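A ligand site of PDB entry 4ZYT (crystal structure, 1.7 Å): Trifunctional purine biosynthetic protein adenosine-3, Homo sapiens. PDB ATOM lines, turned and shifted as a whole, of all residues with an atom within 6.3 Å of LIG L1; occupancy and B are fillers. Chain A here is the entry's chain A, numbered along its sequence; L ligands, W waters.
N of Ile 92 lies within hydrogen-bond range of O5 of LIG L1, at 3.2 Å.
An oxygen (O1) of LIG L1 sits at hydrogen-bond distance from the backbone NH (N) of Asp 145 (3.0 Å).
NE2 of His 59 lies close to O4 of LIG L1.
O of Arg 91 lies within hydrogen-bond range of N3 of LIG L1 (2.9 Å).
The backbone NH (N) of Leu 93 lies within hydrogen-bond range of a nitrogen (N1) of LIG L1, 3.1 Å away.
The backbone carbonyl oxygen (O) of Met 90 lies close to a nitrogen (N5) of LIG L1 (3.1 Å).
The backbone carbonyl oxygen (O) of Ala 141 sits at hydrogen-bond distance from a nitrogen (N2) of LIG L1 (2.8 Å).
NH1 of Arg 91 lies within salt-bridge range of O6 of LIG L1 (3.4 Å).
O5 of LIG L1 lies within salt-bridge range of NH1 of Arg 65 (3.0 Å).
The backbone carbonyl oxygen (O) of Glu 142 lies within hydrogen-bond range of a nitrogen (N4) of LIG L1, at 3.1 Å.
O of Leu 93 lies within hydrogen-bond range of N4 of LIG L1.
N2 of LG2 L2 lies within hydrogen-bond range of O of Gly 118, 3.4 Å away.
NZ of Lys 38 is in salt-bridge range of O4 of LIG L1, 3.4 Å away.
Residues that only touch LIG L1: Leu 86, Phe 89, Val 98, Asn 107, Gly 118, Ser 119, His 138, Val 140, Asp 143 and Val 144.
Hydrophobic or aromatic side chains that line LIG L1: His 59, Leu 86, Met 90, Ile 92, Leu 93, Val 98, His 138, Val 140 and Val 144.
Within 4 Å of LIG L1: Lys 38, His 59, Arg 65, Leu 86, Phe 89, Met 90, Arg 91, Ile 92, Leu 93, Val 98, Asn 107, Gly 118, Ser 119, His 138, Val 140, Ala 141, Glu 142, Asp 143, Val 144 and Asp 145.
The nearest printed residue that does not touch LIG L1 is Asn 37 (4.1 Å).
Water W2 lies within hydrogen-bond range of ND2 of Asn 37, O4 of LIG L1 and O of Met 90.
Water W1 lies within hydrogen-bond range of the side-chain carboxylate of Asp 145 (2.7 Å), a ring nitrogen (ND1) of His 109 (2.7 Å), a nitrogen (N2) of LG2 L2 (2.9 Å) and the side-chain amide nitrogen of Asn 107 (3.0 Å).
ND2 of Asn 37 lies within hydrogen-bond range of ND1 of His 59, at 3.2 Å.
The backbone carbonyl oxygen of His 138 lies within hydrogen-bond range of the backbone NH of Asn 107.
The backbone carbonyl oxygen (O) of Leu 86 sits at hydrogen-bond distance from the backbone NH (N) of Ile 108 (3.4 Å).
The side-chain carboxylate (OD2) of Asp 145 lies close to a ring nitrogen (ND1) of His 109 (3.4 Å).
The side-chain carboxylate (OD2) of Asp 145 is in hydrogen-bond range of the backbone NH (N) of Gly 118, at 2.8 Å.
NH1 of Arg 65 is in hydrogen-bond range of O of Ile 92 (2.7 Å).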
ATOM      1  N   ASN A  37      10.628  -1.865 -25.612  1.00  0.00           N
ATOM      2  CA  ASN A  37       9.474  -2.042 -24.752  1.00  0.00           C
ATOM      3  C   ASN A  37       8.627  -0.767 -24.717  1.00  0.00           C
ATOM      4  O   ASN A  37       7.562  -0.730 -24.090  1.00  0.00           O
ATOM      5  CB  ASN A  37       9.897  -2.442 -23.335  1.00  0.00           C
ATOM      6  CG  ASN A  37      10.670  -1.357 -22.611  1.00  0.00           C
ATOM      7  OD1 ASN A  37      11.602  -0.765 -23.172  1.00  0.00           O
ATOM      8  ND2 ASN A  37      10.297  -1.090 -21.360  1.00  0.00           N
ATOM      9  N   LYS A  38       9.108   0.277 -25.381  1.00  0.00           N
ATOM     10  CA  LYS A  38       8.428   1.558 -25.414  1.00  0.00           C
ATOM     11  C   LYS A  38       8.186   2.019 -26.853  1.00  0.00           C
ATOM     12  O   LYS A  38       9.065   1.928 -27.708  1.00  0.00           O
ATOM     13  CB  LYS A  38       9.233   2.634 -24.667  1.00  0.00           C
ATOM     14  CG  LYS A  38       9.520   2.297 -23.202  1.00  0.00           C
ATOM     15  CD  LYS A  38       8.274   2.356 -22.341  1.00  0.00           C
ATOM     16  CE  LYS A  38       8.630   2.287 -20.860  1.00  0.00           C
ATOM     17  NZ  LYS A  38       7.451   2.496 -19.968  1.00  0.00           N
ATOM     18  N   HIS A  59       5.250  -3.976 -22.533  1.00  0.00           N
ATOM     19  CA  HIS A  59       5.242  -4.774 -21.314  1.00  0.00           C
ATOM     20  C   HIS A  59       3.964  -4.559 -20.521  1.00  0.00           C
ATOM     21  O   HIS A  59       3.596  -5.378 -19.680  1.00  0.00           O
ATOM     22  CB  HIS A  59       6.459  -4.466 -20.437  1.00  0.00           C
ATOM     23  CG  HIS A  59       6.512  -3.048 -19.953  1.00  0.00           C
ATOM     24  ND1 HIS A  59       7.446  -2.136 -20.422  1.00  0.00           N
ATOM     25  CD2 HIS A  59       5.774  -2.383 -19.025  1.00  0.00           C
ATOM     26  CE1 HIS A  59       7.258  -0.971 -19.820  1.00  0.00           C
ATOM     27  NE2 HIS A  59       6.260  -1.100 -18.969  1.00  0.00           N
ATOM     28  N   ARG A  65       6.017 -10.683 -15.841  1.00  0.00           N
ATOM     29  CA  ARG A  65       7.337 -10.536 -16.437  1.00  0.00           C
ATOM     30  C   ARG A  65       7.712 -11.720 -17.340  1.00  0.00           C
ATOM     31  O   ARG A  65       8.301 -11.538 -18.407  1.00  0.00           O
ATOM     32  CB  ARG A  65       8.391 -10.363 -15.333  1.00  0.00           C
ATOM     33  CG  ARG A  65       9.762  -9.906 -15.831  1.00  0.00           C
ATOM     34  CD  ARG A  65      10.686  -9.543 -14.654  1.00  0.00           C
ATOM     35  NE  ARG A  65      10.075  -8.604 -13.714  1.00  0.00           N
ATOM     36  CZ  ARG A  65      10.126  -7.280 -13.831  1.00  0.00           C
ATOM     37  NH1 ARG A  65      10.771  -6.708 -14.837  1.00  0.00           N
ATOM     38  NH2 ARG A  65       9.535  -6.513 -12.916  1.00  0.00           N
ATOM     39  N   LEU A  86      21.547  -5.476 -24.499  1.00  0.00           N
ATOM     40  CA  LEU A  86      20.646  -4.544 -23.821  1.00  0.00           C
ATOM     41  C   LEU A  86      21.287  -3.166 -23.878  1.00  0.00           C
ATOM     42  O   LEU A  86      22.335  -2.945 -23.278  1.00  0.00           O
ATOM     43  CB  LEU A  86      20.397  -4.964 -22.371  1.00  0.00           C
ATOM     44  CG  LEU A  86      19.937  -6.396 -22.126  1.00  0.00           C
ATOM     45  CD1 LEU A  86      19.543  -6.547 -20.659  1.00  0.00           C
ATOM     46  CD2 LEU A  86      18.788  -6.762 -23.034  1.00  0.00           C
ATOM     47  N   PHE A  89      17.978  -0.582 -22.382  1.00  0.00           N
ATOM     48  CA  PHE A  89      16.768  -1.342 -22.083  1.00  0.00           C
ATOM     49  C   PHE A  89      16.555  -1.355 -20.578  1.00  0.00           C
ATOM     50  O   PHE A  89      17.349  -1.944 -19.838  1.00  0.00           O
ATOM     51  CB  PHE A  89      16.900  -2.763 -22.624  1.00  0.00           C
ATOM     52  CG  PHE A  89      15.648  -3.588 -22.490  1.00  0.00           C
ATOM     53  CD1 PHE A  89      14.572  -3.372 -23.338  1.00  0.00           C
ATOM     54  CD2 PHE A  89      15.569  -4.606 -21.554  1.00  0.00           C
ATOM     55  CE1 PHE A  89      13.420  -4.161 -23.225  1.00  0.00           C
ATOM     56  CE2 PHE A  89      14.430  -5.391 -21.441  1.00  0.00           C
ATOM     57  CZ  PHE A  89      13.359  -5.167 -22.280  1.00  0.00           C
ATOM     58  N   MET A  90      15.483  -0.727 -20.117  1.00  0.00           N
ATOM     59  CA  MET A  90      15.317  -0.480 -18.693  1.00  0.00           C
ATOM     60  C   MET A  90      14.259  -1.365 -18.054  1.00  0.00           C
ATOM     61  O   MET A  90      13.331  -0.867 -17.410  1.00  0.00           O
ATOM     62  CB  MET A  90      14.990   0.994 -18.442  1.00  0.00           C
ATOM     63  CG  MET A  90      16.062   1.962 -18.961  1.00  0.00           C
ATOM     64  SD  MET A  90      17.673   1.730 -18.187  1.00  0.00           S
ATOM     65  CE  MET A  90      17.435   2.579 -16.629  1.00  0.00           C
ATOM     66  N   ARG A  91      14.391  -2.673 -18.248  1.00  0.00           N
ATOM     67  CA  ARG A  91      13.542  -3.641 -17.574  1.00  0.00           C
ATOM     68  C   ARG A  91      14.395  -4.760 -16.996  1.00  0.00           C
ATOM     69  O   ARG A  91      15.417  -5.125 -17.564  1.00  0.00           O
ATOM     70  CB  ARG A  91      12.505  -4.240 -18.537  1.00  0.00           C
ATOM     71  CG  ARG A  91      11.405  -3.277 -18.930  1.00  0.00           C
ATOM     72  CD  ARG A  91      10.340  -3.996 -19.726  1.00  0.00           C
ATOM     73  NE  ARG A  91       9.986  -5.273 -19.102  1.00  0.00           N
ATOM     74  CZ  ARG A  91       9.041  -5.429 -18.190  1.00  0.00           C
ATOM     75  NH1 ARG A  91       8.342  -4.390 -17.752  1.00  0.00           N
ATOM     76  NH2 ARG A  91       8.800  -6.642 -17.692  1.00  0.00           N
ATOM     77  N   ILE A  92      13.968  -5.291 -15.860  1.00  0.00           N
ATOM     78  CA  ILE A  92      14.599  -6.484 -15.289  1.00  0.00           C
ATOM     79  C   ILE A  92      14.068  -7.716 -16.016  1.00  0.00           C
ATOM     80  O   ILE A  92      12.863  -7.863 -16.197  1.00  0.00           O
ATOM     81  CB  ILE A  92      14.331  -6.589 -13.784  1.00  0.00           C
ATOM     82  CG1 ILE A  92      15.011  -5.437 -13.045  1.00  0.00           C
ATOM     83  CG2 ILE A  92      14.806  -7.929 -13.235  1.00  0.00           C
ATOM     84  CD1 ILE A  92      14.822  -5.460 -11.553  1.00  0.00           C
ATOM     85  N   LEU A  93      14.977  -8.592 -16.432  1.00  0.00           N
ATOM     86  CA  LEU A  93      14.582  -9.807 -17.131  1.00  0.00           C
ATOM     87  C   LEU A  93      14.378 -10.977 -16.177  1.00  0.00           C
ATOM     88  O   LEU A  93      15.089 -11.095 -15.186  1.00  0.00           O
ATOM     89  CB  LEU A  93      15.619 -10.168 -18.182  1.00  0.00           C
ATOM     90  CG  LEU A  93      15.794  -9.131 -19.285  1.00  0.00           C
ATOM     91  CD1 LEU A  93      17.105  -9.358 -20.011  1.00  0.00           C
ATOM     92  CD2 LEU A  93      14.620  -9.214 -20.238  1.00  0.00           C
ATOM     93  N   SER A  94      13.409 -11.829 -16.496  1.00  0.00           N
ATOM     94  CA  SER A  94      13.086 -12.976 -15.649  1.00  0.00           C
ATOM     95  C   SER A  94      14.181 -14.040 -15.644  1.00  0.00           C
ATOM     96  O   SER A  94      14.960 -14.148 -16.598  1.00  0.00           O
ATOM     97  CB  SER A  94      11.762 -13.605 -16.093  1.00  0.00           C
ATOM     98  OG  SER A  94      11.883 -14.169 -17.395  1.00  0.00           O
ATOM     99  N   GLY A  95      14.213 -14.830 -14.575  1.00  0.00           N
ATOM    100  CA  GLY A  95      15.170 -15.921 -14.445  1.00  0.00           C
ATOM    101  C   GLY A  95      15.293 -16.890 -15.620  1.00  0.00           C
ATOM    102  O   GLY A  95      16.393 -17.139 -16.107  1.00  0.00           O
ATOM    103  N   VAL A  98      16.860 -15.253 -18.689  1.00  0.00           N
ATOM    104  CA  VAL A  98      18.280 -15.032 -18.448  1.00  0.00           C
ATOM    105  C   VAL A  98      19.060 -16.334 -18.558  1.00  0.00           C
ATOM    106  O   VAL A  98      20.130 -16.388 -19.161  1.00  0.00           O
ATOM    107  CB  VAL A  98      18.514 -14.393 -17.062  1.00  0.00           C
ATOM    108  CG1 VAL A  98      19.980 -14.398 -16.695  1.00  0.00           C
ATOM    109  CG2 VAL A  98      17.942 -12.976 -17.049  1.00  0.00           C
ATOM    110  N   ASN A 107      24.953  -6.449 -21.387  1.00  0.00           N
ATOM    111  CA  ASN A 107      24.310  -5.201 -20.936  1.00  0.00           C
ATOM    112  C   ASN A 107      25.331  -4.104 -20.777  1.00  0.00           C
ATOM    113  O   ASN A 107      26.466  -4.388 -20.387  1.00  0.00           O
ATOM    114  CB  ASN A 107      23.578  -5.411 -19.617  1.00  0.00           C
ATOM    115  CG  ASN A 107      22.915  -4.143 -19.112  1.00  0.00           C
ATOM    116  OD1 ASN A 107      22.063  -3.555 -19.802  1.00  0.00           O
ATOM    117  ND2 ASN A 107      23.279  -3.701 -17.906  1.00  0.00           N
ATOM    118  N   ILE A 108      24.955  -2.863 -21.077  1.00  0.00           N
ATOM    119  CA  ILE A 108      25.818  -1.704 -20.786  1.00  0.00           C
ATOM    120  C   ILE A 108      25.241  -0.969 -19.570  1.00  0.00           C
ATOM    121  O   ILE A 108      24.025  -0.767 -19.464  1.00  0.00           O
ATOM    122  CB  ILE A 108      25.971  -0.722 -22.001  1.00  0.00           C
ATOM    123  CG1 ILE A 108      26.885   0.446 -21.660  1.00  0.00           C
ATOM    124  CG2 ILE A 108      24.618  -0.177 -22.444  1.00  0.00           C
ATOM    125  CD1 ILE A 108      28.340   0.154 -21.781  1.00  0.00           C
ATOM    126  N   HIS A 109      26.113  -0.638 -18.636  1.00  0.00           N
ATOM    127  CA  HIS A 109      25.700  -0.011 -17.381  1.00  0.00           C
ATOM    128  C   HIS A 109      26.605   1.182 -17.121  1.00  0.00           C
ATOM    129  O   HIS A 109      27.828   1.056 -17.219  1.00  0.00           O
ATOM    130  CB  HIS A 109      25.767  -1.015 -16.233  1.00  0.00           C
ATOM    131  CG  HIS A 109      25.332  -0.435 -14.923  1.00  0.00           C
ATOM    132  ND1 HIS A 109      24.007  -0.303 -14.575  1.00  0.00           N
ATOM    133  CD2 HIS A 109      26.054   0.083 -13.894  1.00  0.00           C
ATOM    134  CE1 HIS A 109      23.925   0.253 -13.376  1.00  0.00           C
ATOM    135  NE2 HIS A 109      25.149   0.495 -12.944  1.00  0.00           N
ATOM    136  N   GLY A 118      21.941  -0.599 -10.460  1.00  0.00           N
ATOM    137  CA  GLY A 118      20.549  -0.180 -10.499  1.00  0.00           C
ATOM    138  C   GLY A 118      20.231   0.854 -11.561  1.00  0.00           C
ATOM    139  O   GLY A 118      21.038   1.105 -12.451  1.00  0.00           O
ATOM    140  N   SER A 119      19.058   1.462 -11.453  1.00  0.00           N
ATOM    141  CA  SER A 119      18.527   2.270 -12.547  1.00  0.00           C
ATOM    142  C   SER A 119      18.998   3.720 -12.579  1.00  0.00           C
ATOM    143  O   SER A 119      18.768   4.413 -13.561  1.00  0.00           O
ATOM    144  CB  SER A 119      17.000   2.248 -12.500  1.00  0.00           C
ATOM    145  OG  SER A 119      16.560   2.866 -11.305  1.00  0.00           O
ATOM    146  N   HIS A 138      28.760  -6.100 -19.345  1.00  0.00           N
ATOM    147  CA  HIS A 138      28.826  -7.372 -18.636  1.00  0.00           C
ATOM    148  C   HIS A 138      27.833  -8.378 -19.201  1.00  0.00           C
ATOM    149  O   HIS A 138      26.813  -8.018 -19.781  1.00  0.00           O
ATOM    150  CB  HIS A 138      28.546  -7.160 -17.144  1.00  0.00           C
ATOM    151  CG  HIS A 138      27.166  -6.642 -16.849  1.00  0.00           C
ATOM    152  ND1 HIS A 138      26.116  -7.469 -16.535  1.00  0.00           N
ATOM    153  CD2 HIS A 138      26.668  -5.375 -16.846  1.00  0.00           C
ATOM    154  CE1 HIS A 138      25.028  -6.745 -16.341  1.00  0.00           C
ATOM    155  NE2 HIS A 138      25.335  -5.467 -16.521  1.00  0.00           N
ATOM    156  N   PHE A 139      28.139  -9.660 -19.034  1.00  0.00           N
ATOM    157  CA  PHE A 139      27.128 -10.671 -19.308  1.00  0.00           C
ATOM    158  C   PHE A 139      25.982 -10.518 -18.317  1.00  0.00           C
ATOM    159  O   PHE A 139      26.194 -10.210 -17.136  1.00  0.00           O
ATOM    160  CB  PHE A 139      27.723 -12.086 -19.211  1.00  0.00           C
ATOM    161  CG  PHE A 139      28.585 -12.458 -20.382  1.00  0.00           C
ATOM    162  CD1 PHE A 139      28.021 -12.723 -21.633  1.00  0.00           C
ATOM    163  CD2 PHE A 139      29.961 -12.569 -20.231  1.00  0.00           C
ATOM    164  CE1 PHE A 139      28.808 -13.085 -22.703  1.00  0.00           C
ATOM    165  CE2 PHE A 139      30.754 -12.927 -21.308  1.00  0.00           C
ATOM    166  CZ  PHE A 139      30.189 -13.188 -22.542  1.00  0.00           C
ATOM    167  N   VAL A 140      24.762 -10.725 -18.784  1.00  0.00           N
ATOM    168  CA  VAL A 140      23.592 -10.620 -17.931  1.00  0.00           C
ATOM    169  C   VAL A 140      23.332 -11.910 -17.158  1.00  0.00           C
ATOM    170  O   VAL A 140      23.147 -12.981 -17.744  1.00  0.00           O
ATOM    171  CB  VAL A 140      22.345 -10.250 -18.767  1.00  0.00           C
ATOM    172  CG1 VAL A 140      21.068 -10.311 -17.903  1.00  0.00           C
ATOM    173  CG2 VAL A 140      22.535  -8.868 -19.356  1.00  0.00           C
ATOM    174  N   ALA A 141      23.318 -11.805 -15.830  1.00  0.00           N
ATOM    175  CA  ALA A 141      22.977 -12.915 -14.947  1.00  0.00           C
ATOM    176  C   ALA A 141      21.656 -12.580 -14.254  1.00  0.00           C
ATOM    177  O   ALA A 141      21.139 -11.484 -14.443  1.00  0.00           O
ATOM    178  CB  ALA A 141      24.089 -13.145 -13.928  1.00  0.00           C
ATOM    179  N   GLU A 142      21.112 -13.530 -13.502  1.00  0.00           N
ATOM    180  CA  GLU A 142      19.802 -13.363 -12.885  1.00  0.00           C
ATOM    181  C   GLU A 142      19.801 -12.190 -11.920  1.00  0.00           C
ATOM    182  O   GLU A 142      18.879 -11.366 -11.943  1.00  0.00           O
ATOM    183  CB  GLU A 142      19.348 -14.644 -12.177  1.00  0.00           C
ATOM    184  CG  GLU A 142      19.130 -15.822 -13.120  1.00  0.00           C
ATOM    185  CD  GLU A 142      18.242 -16.912 -12.540  1.00  0.00           C
ATOM    186  OE1 GLU A 142      17.352 -16.584 -11.715  1.00  0.00           O
ATOM    187  OE2 GLU A 142      18.422 -18.088 -12.921  1.00  0.00           O
ATOM    188  N   ASP A 143      20.815 -12.095 -11.073  1.00  0.00           N
ATOM    189  CA  ASP A 143      20.969 -10.930 -10.209  1.00  0.00           C
ATOM    190  C   ASP A 143      21.366  -9.737 -11.064  1.00  0.00           C
ATOM    191  O   ASP A 143      22.255  -9.837 -11.915  1.00  0.00           O
ATOM    192  CB  ASP A 143      21.999 -11.178  -9.113  1.00  0.00           C
ATOM    193  CG  ASP A 143      21.461 -12.059  -8.006  1.00  0.00           C
ATOM    194  OD1 ASP A 143      20.231 -12.182  -7.887  1.00  0.00           O
ATOM    195  OD2 ASP A 143      22.282 -12.613  -7.250  1.00  0.00           O
ATOM    196  N   VAL A 144      20.712  -8.606 -10.826  1.00  0.00           N
ATOM    197  CA  VAL A 144      20.898  -7.423 -11.670  1.00  0.00           C
ATOM    198  C   VAL A 144      22.252  -6.754 -11.484  1.00  0.00           C
ATOM    199  O   VAL A 144      22.686  -6.505 -10.359  1.00  0.00           O
ATOM    200  CB  VAL A 144      19.780  -6.392 -11.407  1.00  0.00           C
ATOM    201  CG1 VAL A 144      20.016  -5.124 -12.201  1.00  0.00           C
ATOM    202  CG2 VAL A 144      18.433  -6.990 -11.766  1.00  0.00           C
ATOM    203  N   ASP A 145      22.921  -6.495 -12.611  1.00  0.00           N
ATOM    204  CA  ASP A 145      24.237  -5.858 -12.654  1.00  0.00           C
ATOM    205  C   ASP A 145      25.307  -6.631 -11.910  1.00  0.00           C
ATOM    206  O   ASP A 145      26.301  -6.058 -11.457  1.00  0.00           O
ATOM    207  CB  ASP A 145      24.143  -4.416 -12.110  1.00  0.00           C
ATOM    208  CG  ASP A 145      23.218  -3.538 -12.941  1.00  0.00           C
ATOM    209  OD1 ASP A 145      22.988  -3.859 -14.132  1.00  0.00           O
ATOM    210  OD2 ASP A 145      22.711  -2.520 -12.404  1.00  0.00           O
ATOM    211  N   ALA A 146      25.137  -7.952 -11.809  1.00  0.00           N
ATOM    212  CA  ALA A 146      26.091  -8.784 -11.087  1.00  0.00           C
ATOM    213  C   ALA A 146      26.809  -9.806 -11.981  1.00  0.00           C
ATOM    214  O   ALA A 146      27.668 -10.552 -11.497  1.00  0.00           O
ATOM    215  CB  ALA A 146      25.393  -9.520  -9.933  1.00  0.00           C
ATOM    216  N   GLY A 147      26.459  -9.847 -13.259  1.00  0.00           N
ATOM    217  CA  GLY A 147      27.052 -10.798 -14.179  1.00  0.00           C
ATOM    218  C   GLY A 147      28.502 -10.505 -14.513  1.00  0.00           C
ATOM    219  O   GLY A 147      29.043  -9.448 -14.161  1.00  0.00           O
HETATM  220  C1  LIG L   1      15.390  -1.952 -12.663  1.00  0.00           C
HETATM  221  C2  LIG L   1      16.752  -1.932 -12.946  1.00  0.00           C
HETATM  222  C3  LIG L   1      12.965  -1.407 -13.346  1.00  0.00           C
HETATM  223  C4  LIG L   1      10.772  -1.472 -14.582  1.00  0.00           C
HETATM  224  C5  LIG L   1      10.258  -0.804 -15.832  1.00  0.00           C
HETATM  225  N1  LIG L   1      17.948  -8.163 -15.736  1.00  0.00           N
HETATM  226  C6  LIG L   1      19.024  -4.986 -17.016  1.00  0.00           C
HETATM  227  C7  LIG L   1      20.137  -5.588 -16.483  1.00  0.00           C
HETATM  228  C8  LIG L   1      19.917  -6.845 -15.934  1.00  0.00           C
HETATM  229  C9  LIG L   1      18.535  -7.018 -16.157  1.00  0.00           C
HETATM  230  C10 LIG L   1      14.950  -0.845 -14.760  1.00  0.00           C
HETATM  231  C11 LIG L   1      16.298  -0.829 -15.043  1.00  0.00           C
HETATM  232  C12 LIG L   1      18.650  -9.119 -15.122  1.00  0.00           C
HETATM  233  N2  LIG L   1      19.967  -8.976 -14.901  1.00  0.00           N
HETATM  234  C13 LIG L   1      20.609  -7.868 -15.295  1.00  0.00           C
HETATM  235  N3  LIG L   1      18.085  -5.918 -16.783  1.00  0.00           N
HETATM  236  O1  LIG L   1      21.818  -7.783 -15.059  1.00  0.00           O
HETATM  237  N4  LIG L   1      18.013 -10.316 -14.689  1.00  0.00           N
HETATM  238  C14 LIG L   1      14.491  -1.391 -13.572  1.00  0.00           C
HETATM  239  O2  LIG L   1      12.473  -1.466 -12.235  1.00  0.00           O
HETATM  240  N5  LIG L   1      12.193  -1.414 -14.539  1.00  0.00           N
HETATM  241  C15 LIG L   1      10.329   0.709 -15.745  1.00  0.00           C
HETATM  242  C16 LIG L   1       9.479   1.271 -16.874  1.00  0.00           C
HETATM  243  O3  LIG L   1       9.157   2.491 -16.873  1.00  0.00           O
HETATM  244  O4  LIG L   1       9.095   0.511 -17.805  1.00  0.00           O
HETATM  245  C17 LIG L   1      10.415  -2.940 -14.693  1.00  0.00           C
HETATM  246  O5  LIG L   1      11.337  -3.799 -14.793  1.00  0.00           O
HETATM  247  O6  LIG L   1       9.209  -3.301 -14.695  1.00  0.00           O
HETATM  248  C18 LIG L   1      18.873  -3.625 -17.673  1.00  0.00           C
HETATM  249  C19 LIG L   1      18.285  -2.636 -16.668  1.00  0.00           C
HETATM  250  C20 LIG L   1      19.171  -2.441 -15.450  1.00  0.00           C
HETATM  251  C21 LIG L   1      18.663  -1.353 -14.504  1.00  0.00           C
HETATM  252  C22 LIG L   1      17.204  -1.364 -14.141  1.00  0.00           C
HETATM  253  C1  LG2 L   2      22.967   4.552 -21.268  1.00  0.00           C
HETATM  254  O1  LG2 L   2      23.712   5.509 -20.514  1.00  0.00           O
HETATM  255  C2  LG2 L   2      23.030   3.217 -20.571  1.00  0.00           C
HETATM  256  O2  LG2 L   2      24.312   2.914 -20.031  1.00  0.00           O
HETATM  257  C3  LG2 L   2      21.994   3.400 -19.478  1.00  0.00           C
HETATM  258  O3  LG2 L   2      20.926   4.045 -20.165  1.00  0.00           O
HETATM  259  C4  LG2 L   2      21.489   4.892 -21.182  1.00  0.00           C
HETATM  260  C5  LG2 L   2      20.819   4.610 -22.508  1.00  0.00           C
HETATM  261  O4  LG2 L   2      21.172   5.624 -23.451  1.00  0.00           O
HETATM  262  N1  LG2 L   2      21.592   2.137 -18.905  1.00  0.00           N
HETATM  263  C6  LG2 L   2      21.295   2.022 -17.623  1.00  0.00           C
HETATM  264  O5  LG2 L   2      21.212   2.986 -16.856  1.00  0.00           O
HETATM  265  C7  LG2 L   2      21.040   0.602 -17.172  1.00  0.00           C
HETATM  266  N2  LG2 L   2      20.665   0.533 -15.772  1.00  0.00           N
HETATM  267  P1  LG2 L   2      20.895   5.375 -25.024  1.00  0.00           P
HETATM  268  O6  LG2 L   2      21.300   6.699 -25.646  1.00  0.00           O
HETATM  269  O7  LG2 L   2      19.422   5.065 -25.146  1.00  0.00           O
HETATM  270  O8  LG2 L   2      21.748   4.189 -25.381  1.00  0.00           O
HETATM  271  O   HOH W   1      22.201  -1.930 -15.783  1.00  0.00           O
HETATM  272  O   HOH W   2      11.552   0.760 -19.439  1.00  0.00           O
HETATM  273  O   HOH W   3      23.750  -9.500 -14.152  1.00  0.00           O
